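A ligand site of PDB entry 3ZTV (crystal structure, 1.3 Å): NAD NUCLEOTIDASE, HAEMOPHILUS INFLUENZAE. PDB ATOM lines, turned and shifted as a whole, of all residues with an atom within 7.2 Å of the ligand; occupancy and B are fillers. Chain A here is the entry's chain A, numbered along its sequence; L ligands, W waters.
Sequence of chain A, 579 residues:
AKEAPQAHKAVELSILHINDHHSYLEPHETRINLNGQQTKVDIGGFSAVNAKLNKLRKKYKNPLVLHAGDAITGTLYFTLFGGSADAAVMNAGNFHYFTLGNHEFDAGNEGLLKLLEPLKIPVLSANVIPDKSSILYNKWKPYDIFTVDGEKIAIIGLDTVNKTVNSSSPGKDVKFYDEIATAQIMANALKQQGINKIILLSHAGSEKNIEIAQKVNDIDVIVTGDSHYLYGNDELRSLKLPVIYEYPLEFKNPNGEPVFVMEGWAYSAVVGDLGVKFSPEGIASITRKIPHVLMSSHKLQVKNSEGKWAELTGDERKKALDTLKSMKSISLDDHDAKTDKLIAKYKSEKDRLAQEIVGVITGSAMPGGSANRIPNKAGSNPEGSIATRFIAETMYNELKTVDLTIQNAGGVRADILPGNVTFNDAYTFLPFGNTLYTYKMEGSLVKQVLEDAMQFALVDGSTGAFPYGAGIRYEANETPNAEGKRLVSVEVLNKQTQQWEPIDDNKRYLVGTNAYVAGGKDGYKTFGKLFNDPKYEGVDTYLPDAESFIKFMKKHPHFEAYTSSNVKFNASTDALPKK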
ATOM      1  N   ARG A 373      -2.746  12.953  -4.245  1.00  0.00           N
ATOM      2  CA  ARG A 373      -3.451  11.700  -4.023  1.00  0.00           C
ATOM      3  C   ARG A 373      -3.262  11.132  -2.619  1.00  0.00           C
ATOM      4  O   ARG A 373      -4.218  10.624  -2.023  1.00  0.00           O
ATOM      5  CB  ARG A 373      -3.052  10.655  -5.064  1.00  0.00           C
ATOM      6  CG  ARG A 373      -3.648  10.900  -6.433  1.00  0.00           C
ATOM      7  CD  ARG A 373      -3.045   9.962  -7.462  1.00  0.00           C
ATOM      8  NE  ARG A 373      -3.688  10.096  -8.770  1.00  0.00           N
ATOM      9  CZ  ARG A 373      -3.321   9.406  -9.837  1.00  0.00           C
ATOM     10  NH1 ARG A 373      -2.340   8.520  -9.744  1.00  0.00           N
ATOM     11  NH2 ARG A 373      -3.954   9.575 -10.998  1.00  0.00           N
ATOM     12  N   GLN A 407     -14.543   7.222  -2.253  1.00  0.00           N
ATOM     13  CA  GLN A 407     -14.113   7.637  -3.594  1.00  0.00           C
ATOM     14  C   GLN A 407     -12.597   7.514  -3.704  1.00  0.00           C
ATOM     15  O   GLN A 407     -11.876   7.832  -2.759  1.00  0.00           O
ATOM     16  CB  GLN A 407     -14.557   9.083  -3.891  1.00  0.00           C
ATOM     17  CG  GLN A 407     -14.072   9.670  -5.225  1.00  0.00           C
ATOM     18  CD  GLN A 407     -14.776   9.093  -6.441  1.00  0.00           C
ATOM     19  OE1 GLN A 407     -15.664   8.256  -6.333  1.00  0.00           O
ATOM     20  NE2 GLN A 407     -14.374   9.553  -7.621  1.00  0.00           N
ATOM     21  N   ASN A 408     -12.108   7.025  -4.839  1.00  0.00           N
ATOM     22  CA  ASN A 408     -10.664   6.916  -5.077  1.00  0.00           C
ATOM     23  C   ASN A 408     -10.076   8.227  -5.588  1.00  0.00           C
ATOM     24  O   ASN A 408     -10.679   8.902  -6.428  1.00  0.00           O
ATOM     25  CB  ASN A 408     -10.364   5.775  -6.057  1.00  0.00           C
ATOM     26  CG  ASN A 408     -10.944   6.027  -7.440  1.00  0.00           C
ATOM     27  OD1 ASN A 408     -12.150   6.232  -7.599  1.00  0.00           O
ATOM     28  ND2 ASN A 408     -10.078   6.029  -8.442  1.00  0.00           N
ATOM     29  N   ALA A 409      -8.892   8.587  -5.081  1.00  0.00           N
ATOM     30  CA  ALA A 409      -8.243   9.865  -5.415  1.00  0.00           C
ATOM     31  C   ALA A 409      -7.967  10.043  -6.915  1.00  0.00           C
ATOM     32  O   ALA A 409      -7.922  11.167  -7.401  1.00  0.00           O
ATOM     33  CB  ALA A 409      -6.951  10.022  -4.608  1.00  0.00           C
ATOM     34  N   GLY A 410      -7.773   8.950  -7.623  1.00  0.00           N
ATOM     35  CA  GLY A 410      -7.507   9.019  -9.056  1.00  0.00           C
ATOM     36  C   GLY A 410      -8.717   9.449  -9.866  1.00  0.00           C
ATOM     37  O   GLY A 410      -8.605   9.729 -11.063  1.00  0.00           O
ATOM     38  N   GLY A 411      -9.871   9.501  -9.211  1.00  0.00           N
ATOM     39  CA  GLY A 411     -11.098   9.899  -9.881  1.00  0.00           C
ATOM     40  C   GLY A 411     -11.272  11.408  -9.925  1.00  0.00           C
ATOM     41  O   GLY A 411     -12.269  11.911 -10.450  1.00  0.00           O
ATOM     42  N   VAL A 412     -10.300  12.130  -9.373  1.00  0.00           N
ATOM     43  CA  VAL A 412     -10.305  13.581  -9.374  1.00  0.00           C
ATOM     44  C   VAL A 412      -8.978  14.100  -9.955  1.00  0.00           C
ATOM     45  O   VAL A 412      -7.906  13.840  -9.394  1.00  0.00           O
ATOM     46  CB  VAL A 412     -10.586  14.158  -7.959  1.00  0.00           C
ATOM     47  CG1 VAL A 412     -11.677  13.354  -7.280  1.00  0.00           C
ATOM     48  CG2 VAL A 412      -9.323  14.148  -7.113  1.00  0.00           C
ATOM     49  N   ARG A 413      -9.047  14.805 -11.077  1.00  0.00           N
ATOM     50  CA  ARG A 413      -7.864  15.081 -11.888  1.00  0.00           C
ATOM     51  C   ARG A 413      -7.159  16.399 -11.607  1.00  0.00           C
ATOM     52  O   ARG A 413      -6.091  16.654 -12.156  1.00  0.00           O
ATOM     53  CB  ARG A 413      -8.223  15.023 -13.385  1.00  0.00           C
ATOM     54  CG  ARG A 413      -8.377  13.634 -13.950  1.00  0.00           C
ATOM     55  CD  ARG A 413      -8.672  13.701 -15.433  1.00  0.00           C
ATOM     56  NE  ARG A 413      -8.349  12.465 -16.126  1.00  0.00           N
ATOM     57  CZ  ARG A 413      -8.638  12.229 -17.409  1.00  0.00           C
ATOM     58  NH1 ARG A 413      -9.287  13.150 -18.116  1.00  0.00           N
ATOM     59  NH2 ARG A 413      -8.308  11.081 -17.967  1.00  0.00           N
ATOM     60  N   PRO A 431     -14.724  13.329 -15.549  1.00  0.00           N
ATOM     61  CA  PRO A 431     -14.758  12.947 -16.962  1.00  0.00           C
ATOM     62  C   PRO A 431     -14.956  11.458 -17.246  1.00  0.00           C
ATOM     63  O   PRO A 431     -15.013  11.079 -18.415  1.00  0.00           O
ATOM     64  CB  PRO A 431     -13.376  13.373 -17.451  1.00  0.00           C
ATOM     65  CG  PRO A 431     -12.495  13.094 -16.270  1.00  0.00           C
ATOM     66  CD  PRO A 431     -13.341  13.394 -15.039  1.00  0.00           C
ATOM     67  N   PHE A 432     -15.054  10.629 -16.208  1.00  0.00           N
ATOM     68  CA  PHE A 432     -15.029   9.175 -16.404  1.00  0.00           C
ATOM     69  C   PHE A 432     -16.393   8.521 -16.647  1.00  0.00           C
ATOM     70  O   PHE A 432     -16.460   7.375 -17.086  1.00  0.00           O
ATOM     71  CB  PHE A 432     -14.324   8.496 -15.230  1.00  0.00           C
ATOM     72  CG  PHE A 432     -12.847   8.779 -15.167  1.00  0.00           C
ATOM     73  CD1 PHE A 432     -12.002   8.314 -16.165  1.00  0.00           C
ATOM     74  CD2 PHE A 432     -12.309   9.488 -14.110  1.00  0.00           C
ATOM     75  CE1 PHE A 432     -10.636   8.562 -16.101  1.00  0.00           C
ATOM     76  CE2 PHE A 432     -10.953   9.744 -14.047  1.00  0.00           C
ATOM     77  CZ  PHE A 432     -10.112   9.287 -15.038  1.00  0.00           C
ATOM     78  N   GLY A 433     -17.463   9.248 -16.355  1.00  0.00           N
ATOM     79  CA  GLY A 433     -18.801   8.730 -16.571  1.00  0.00           C
ATOM     80  C   GLY A 433     -19.244   7.636 -15.604  1.00  0.00           C
ATOM     81  O   GLY A 433     -20.018   6.757 -15.966  1.00  0.00           O
ATOM     82  N   ASN A 434     -18.764   7.700 -14.363  1.00  0.00           N
ATOM     83  CA  ASN A 434     -19.200   6.741 -13.349  1.00  0.00           C
ATOM     84  C   ASN A 434     -20.614   7.021 -12.873  1.00  0.00           C
ATOM     85  O   ASN A 434     -21.081   8.163 -12.940  1.00  0.00           O
ATOM     86  CB  ASN A 434     -18.284   6.769 -12.131  1.00  0.00           C
ATOM     87  CG  ASN A 434     -16.876   6.350 -12.436  1.00  0.00           C
ATOM     88  OD1 ASN A 434     -16.628   5.452 -13.247  1.00  0.00           O
ATOM     89  ND2 ASN A 434     -15.915   7.009 -11.787  1.00  0.00           N
ATOM     90  N   PHE A 456      -2.904  -0.993  -2.558  1.00  0.00           N
ATOM     91  CA  PHE A 456      -2.711  -0.777  -3.991  1.00  0.00           C
ATOM     92  C   PHE A 456      -2.045   0.585  -4.229  1.00  0.00           C
ATOM     93  O   PHE A 456      -1.115   0.694  -5.031  1.00  0.00           O
ATOM     94  CB  PHE A 456      -4.053  -0.857  -4.737  1.00  0.00           C
ATOM     95  CG  PHE A 456      -3.926  -1.078  -6.228  1.00  0.00           C
ATOM     96  CD1 PHE A 456      -3.693  -2.343  -6.733  1.00  0.00           C
ATOM     97  CD2 PHE A 456      -4.086  -0.027  -7.110  1.00  0.00           C
ATOM     98  CE1 PHE A 456      -3.580  -2.550  -8.101  1.00  0.00           C
ATOM     99  CE2 PHE A 456      -3.981  -0.232  -8.485  1.00  0.00           C
ATOM    100  CZ  PHE A 456      -3.731  -1.496  -8.963  1.00  0.00           C
ATOM    101  N   GLY A 461       0.149  -0.875  -6.872  1.00  0.00           N
ATOM    102  CA  GLY A 461      -0.341  -0.237  -8.076  1.00  0.00           C
ATOM    103  C   GLY A 461      -0.374   1.291  -8.084  1.00  0.00           C
ATOM    104  O   GLY A 461       0.521   1.940  -7.547  1.00  0.00           O
ATOM    105  N   SER A 462      -1.414   1.835  -8.699  1.00  0.00           N
ATOM    106  CA  SER A 462      -1.564   3.271  -8.908  1.00  0.00           C
ATOM    107  C   SER A 462      -1.930   4.025  -7.633  1.00  0.00           C
ATOM    108  O   SER A 462      -2.793   3.589  -6.878  1.00  0.00           O
ATOM    109  CB  SER A 462      -2.621   3.531  -9.985  1.00  0.00           C
ATOM    110  OG  SER A 462      -3.032   4.882 -10.005  1.00  0.00           O
ATOM    111  N   THR A 463      -1.281   5.166  -7.418  1.00  0.00           N
ATOM    112  CA  THR A 463      -1.596   6.008  -6.259  1.00  0.00           C
ATOM    113  C   THR A 463      -3.028   6.505  -6.319  1.00  0.00           C
ATOM    114  O   THR A 463      -3.576   6.956  -5.311  1.00  0.00           O
ATOM    115  CB  THR A 463      -0.653   7.222  -6.182  1.00  0.00           C
ATOM    116  OG1 THR A 463      -0.670   7.924  -7.431  1.00  0.00           O
ATOM    117  CG2 THR A 463       0.766   6.775  -5.858  1.00  0.00           C
ATOM    118  N   GLY A 464      -3.645   6.423  -7.496  1.00  0.00           N
ATOM    119  CA  GLY A 464      -5.020   6.869  -7.659  1.00  0.00           C
ATOM    120  C   GLY A 464      -6.036   6.053  -6.869  1.00  0.00           C
ATOM    121  O   GLY A 464      -7.198   6.446  -6.769  1.00  0.00           O
ATOM    122  N   ALA A 465      -5.610   4.920  -6.331  1.00  0.00           N
ATOM    123  CA  ALA A 465      -6.502   4.078  -5.530  1.00  0.00           C
ATOM    124  C   ALA A 465      -6.764   4.633  -4.126  1.00  0.00           C
ATOM    125  O   ALA A 465      -7.685   4.187  -3.446  1.00  0.00           O
ATOM    126  CB  ALA A 465      -5.951   2.659  -5.425  1.00  0.00           C
ATOM    127  N   PHE A 466      -5.954   5.596  -3.689  1.00  0.00           N
ATOM    128  CA  PHE A 466      -6.036   6.026  -2.289  1.00  0.00           C
ATOM    129  C   PHE A 466      -7.441   6.519  -1.951  1.00  0.00           C
ATOM    130  O   PHE A 466      -7.975   7.393  -2.644  1.00  0.00           O
ATOM    131  CB  PHE A 466      -4.980   7.081  -1.977  1.00  0.00           C
ATOM    132  CG  PHE A 466      -4.712   7.205  -0.499  1.00  0.00           C
ATOM    133  CD1 PHE A 466      -5.501   8.016   0.291  1.00  0.00           C
ATOM    134  CD2 PHE A 466      -3.681   6.479   0.087  1.00  0.00           C
ATOM    135  CE1 PHE A 466      -5.278   8.121   1.648  1.00  0.00           C
ATOM    136  CE2 PHE A 466      -3.450   6.582   1.451  1.00  0.00           C
ATOM    137  CZ  PHE A 466      -4.251   7.410   2.229  1.00  0.00           C
ATOM    138  N   ASN A 514     -18.143   4.585  -6.482  1.00  0.00           N
ATOM    139  CA  ASN A 514     -18.361   4.729  -7.920  1.00  0.00           C
ATOM    140  C   ASN A 514     -18.322   3.357  -8.593  1.00  0.00           C
ATOM    141  O   ASN A 514     -17.758   2.407  -8.057  1.00  0.00           O
ATOM    142  CB  ASN A 514     -17.369   5.708  -8.564  1.00  0.00           C
ATOM    143  CG  ASN A 514     -15.948   5.205  -8.554  1.00  0.00           C
ATOM    144  OD1 ASN A 514     -15.643   4.191  -9.164  1.00  0.00           O
ATOM    145  ND2 ASN A 514     -15.067   5.927  -7.863  1.00  0.00           N
ATOM    146  N   ALA A 515     -18.942   3.260  -9.772  1.00  0.00           N
ATOM    147  CA  ALA A 515     -19.085   1.997 -10.473  1.00  0.00           C
ATOM    148  C   ALA A 515     -17.751   1.345 -10.843  1.00  0.00           C
ATOM    149  O   ALA A 515     -17.644   0.128 -10.909  1.00  0.00           O
ATOM    150  CB  ALA A 515     -19.934   2.186 -11.714  1.00  0.00           C
ATOM    151  N   TYR A 516     -16.734   2.173 -11.071  1.00  0.00           N
ATOM    152  CA  TYR A 516     -15.397   1.694 -11.437  1.00  0.00           C
ATOM    153  C   TYR A 516     -14.781   0.855 -10.319  1.00  0.00           C
ATOM    154  O   TYR A 516     -14.458  -0.308 -10.521  1.00  0.00           O
ATOM    155  CB  TYR A 516     -14.523   2.896 -11.820  1.00  0.00           C
ATOM    156  CG  TYR A 516     -13.045   2.625 -12.066  1.00  0.00           C
ATOM    157  CD1 TYR A 516     -12.585   2.138 -13.288  1.00  0.00           C
ATOM    158  CD2 TYR A 516     -12.106   2.922 -11.088  1.00  0.00           C
ATOM    159  CE1 TYR A 516     -11.230   1.930 -13.506  1.00  0.00           C
ATOM    160  CE2 TYR A 516     -10.754   2.712 -11.289  1.00  0.00           C
ATOM    161  CZ  TYR A 516     -10.322   2.213 -12.499  1.00  0.00           C
ATOM    162  OH  TYR A 516      -8.974   2.010 -12.693  1.00  0.00           O
ATOM    163  N   VAL A 517     -14.621   1.432  -9.127  1.00  0.00           N
ATOM    164  CA  VAL A 517     -14.059   0.626  -8.033  1.00  0.00           C
ATOM    165  C   VAL A 517     -15.037  -0.409  -7.463  1.00  0.00           C
ATOM    166  O   VAL A 517     -14.614  -1.394  -6.849  1.00  0.00           O
ATOM    167  CB  VAL A 517     -13.468   1.497  -6.894  1.00  0.00           C
ATOM    168  CG1 VAL A 517     -12.353   2.378  -7.430  1.00  0.00           C
ATOM    169  CG2 VAL A 517     -14.541   2.329  -6.230  1.00  0.00           C
ATOM    170  N   LYS A 521     -11.831  -2.619  -9.491  1.00  0.00           N
ATOM    171  CA  LYS A 521     -10.711  -1.933 -10.133  1.00  0.00           C
ATOM    172  C   LYS A 521      -9.891  -1.158  -9.098  1.00  0.00           C
ATOM    173  O   LYS A 521     -10.352  -0.939  -7.968  1.00  0.00           O
ATOM    174  CB  LYS A 521     -11.209  -1.003 -11.244  1.00  0.00           C
ATOM    175  CG  LYS A 521     -12.022  -1.693 -12.320  1.00  0.00           C
ATOM    176  CD  LYS A 521     -11.166  -2.607 -13.164  1.00  0.00           C
ATOM    177  CE  LYS A 521     -12.019  -3.375 -14.162  1.00  0.00           C
ATOM    178  NZ  LYS A 521     -12.931  -2.455 -14.905  1.00  0.00           N
ATOM    179  N   ASP A 522      -8.686  -0.751  -9.483  1.00  0.00           N
ATOM    180  CA  ASP A 522      -7.792  -0.009  -8.594  1.00  0.00           C
ATOM    181  C   ASP A 522      -7.493  -0.764  -7.300  1.00  0.00           C
ATOM    182  O   ASP A 522      -7.252  -0.155  -6.256  1.00  0.00           O
ATOM    183  CB  ASP A 522      -8.348   1.381  -8.291  1.00  0.00           C
ATOM    184  CG  ASP A 522      -7.511   2.507  -8.907  1.00  0.00           C
ATOM    185  OD1 ASP A 522      -6.622   2.201  -9.743  1.00  0.00           O
ATOM    186  OD2 ASP A 522      -7.728   3.678  -8.564  1.00  0.00           O
ATOM    187  N   ASP A 545     -22.106  10.635 -11.880  1.00  0.00           N
ATOM    188  CA  ASP A 545     -21.220  11.410 -11.017  1.00  0.00           C
ATOM    189  C   ASP A 545     -21.257  12.930 -11.215  1.00  0.00           C
ATOM    190  O   ASP A 545     -21.359  13.684 -10.245  1.00  0.00           O
ATOM    191  CB  ASP A 545     -19.767  10.887 -11.045  1.00  0.00           C
ATOM    192  CG  ASP A 545     -19.189  10.736 -12.454  1.00  0.00           C
ATOM    193  OD1 ASP A 545     -19.793  11.229 -13.435  1.00  0.00           O
ATOM    194  OD2 ASP A 545     -18.110  10.113 -12.579  1.00  0.00           O
HETATM  195  O1  LIG L   1      -4.676   6.762 -14.739  1.00  0.00           O
HETATM  196  C1  LIG L   1      -5.277   5.583 -14.191  1.00  0.00           C
HETATM  197  C2  LIG L   1      -5.916   5.948 -12.848  1.00  0.00           C
HETATM  198  O2  LIG L   1      -7.028   6.818 -13.058  1.00  0.00           O
HETATM  199  C3  LIG L   1      -6.453   4.740 -12.110  1.00  0.00           C
HETATM  200  O3  LIG L   1      -5.460   4.181 -11.245  1.00  0.00           O
HETATM  201  C4  LIG L   1      -7.617   5.322 -11.321  1.00  0.00           C
HETATM  202  O4  LIG L   1      -7.179   5.822 -10.058  1.00  0.00           O
HETATM  203  C5  LIG L   1      -8.096   6.478 -12.166  1.00  0.00           C
HETATM  204  N1  LIG L   1      -9.281   6.071 -12.950  1.00  0.00           N
HETATM  205  C6  LIG L   1      -9.303   5.547 -14.195  1.00  0.00           C
HETATM  206  N2  LIG L   1     -10.583   5.292 -14.588  1.00  0.00           N
HETATM  207  C7  LIG L   1     -11.400   5.656 -13.574  1.00  0.00           C
HETATM  208  C8  LIG L   1     -12.849   5.661 -13.303  1.00  0.00           C
HETATM  209  N3  LIG L   1     -13.755   5.219 -14.211  1.00  0.00           N
HETATM  210  N4  LIG L   1     -13.268   6.130 -12.100  1.00  0.00           N
HETATM  211  C9  LIG L   1     -12.404   6.589 -11.173  1.00  0.00           C
HETATM  212  N5  LIG L   1     -11.082   6.604 -11.351  1.00  0.00           N
HETATM  213  C10 LIG L   1     -10.532   6.167 -12.505  1.00  0.00           C
HETATM  214  O   HOH W   1     -10.983   4.261 -17.147  1.00  0.00           O
HETATM  215  O   HOH W   2     -13.645   4.179 -16.906  1.00  0.00           O
HETATM  216  O   HOH W   3      -6.607  10.168 -13.041  1.00  0.00           O
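Water W3 lies within hydrogen-bond range of the backbone carbonyl oxygen of Gly 410 (2.8 Å), an oxygen (O2) of the ligand (3.4 Å) and the guanidinium group of Arg 373 (3.4 Å).
The side-chain amide nitrogen (ND2) of Asn 408 lies within hydrogen-bond range of the side-chain carboxylate (OD2) of Asp 522.
N of Ala 465 lies close to OD2 of Asp 522, at 3.3 Å.
N of Asp 545 sits at hydrogen-bond distance from O of Asn 434, 2.9 Å away.
ND2 of Asn 408 lies close to O of Gly 464 (3.4 Å).
ND2 of Asn 514 sits at hydrogen-bond distance from OD1 of Asn 408 (2.9 Å).
The backbone NH of Tyr 516 is in hydrogen-bond range of the side-chain amide oxygen of Asn 514, at 3.0 Å.
N of Gly 410 is in hydrogen-bond range of O of Gly 464.
The backbone carbonyl oxygen (O) of Gly 464 is in hydrogen-bond range of the backbone NH (N) of Ala 409 (3.2 Å).
Merely in contact with the ligand: Tyr 516 (3.3 Å), Gly 410 (3.4 Å), Phe 432 (3.5 Å) and Gly 411 (3.6 Å).
Hydrophobic or aromatic side chains within 4 Å of the ligand: Phe 432 and Tyr 516.
Nine residues have an atom within 4 Å of the ligand: Asn 408, Gly 410, Gly 411, Phe 432, Asn 434, Ser 462, Gly 464, Tyr 516 and Asp 522.
The side-chain carboxylate of Asp 522 is in hydrogen-bond range of an oxygen (O4) of the ligand (2.7 Å).
ND2 of Asn 434 is in hydrogen-bond range of N4 of the ligand (2.8 Å).
An oxygen (O3) of the ligand sits at hydrogen-bond distance from the side-chain hydroxyl (OG) of Ser 462 (2.8 Å).
The side-chain amide nitrogen of Asn 408 lies within hydrogen-bond range of a nitrogen (N5) of the ligand, 3.1 Å away.
An oxygen (O4) of the ligand lies within hydrogen-bond range of the backbone carbonyl oxygen of Gly 464 (3.3 Å).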
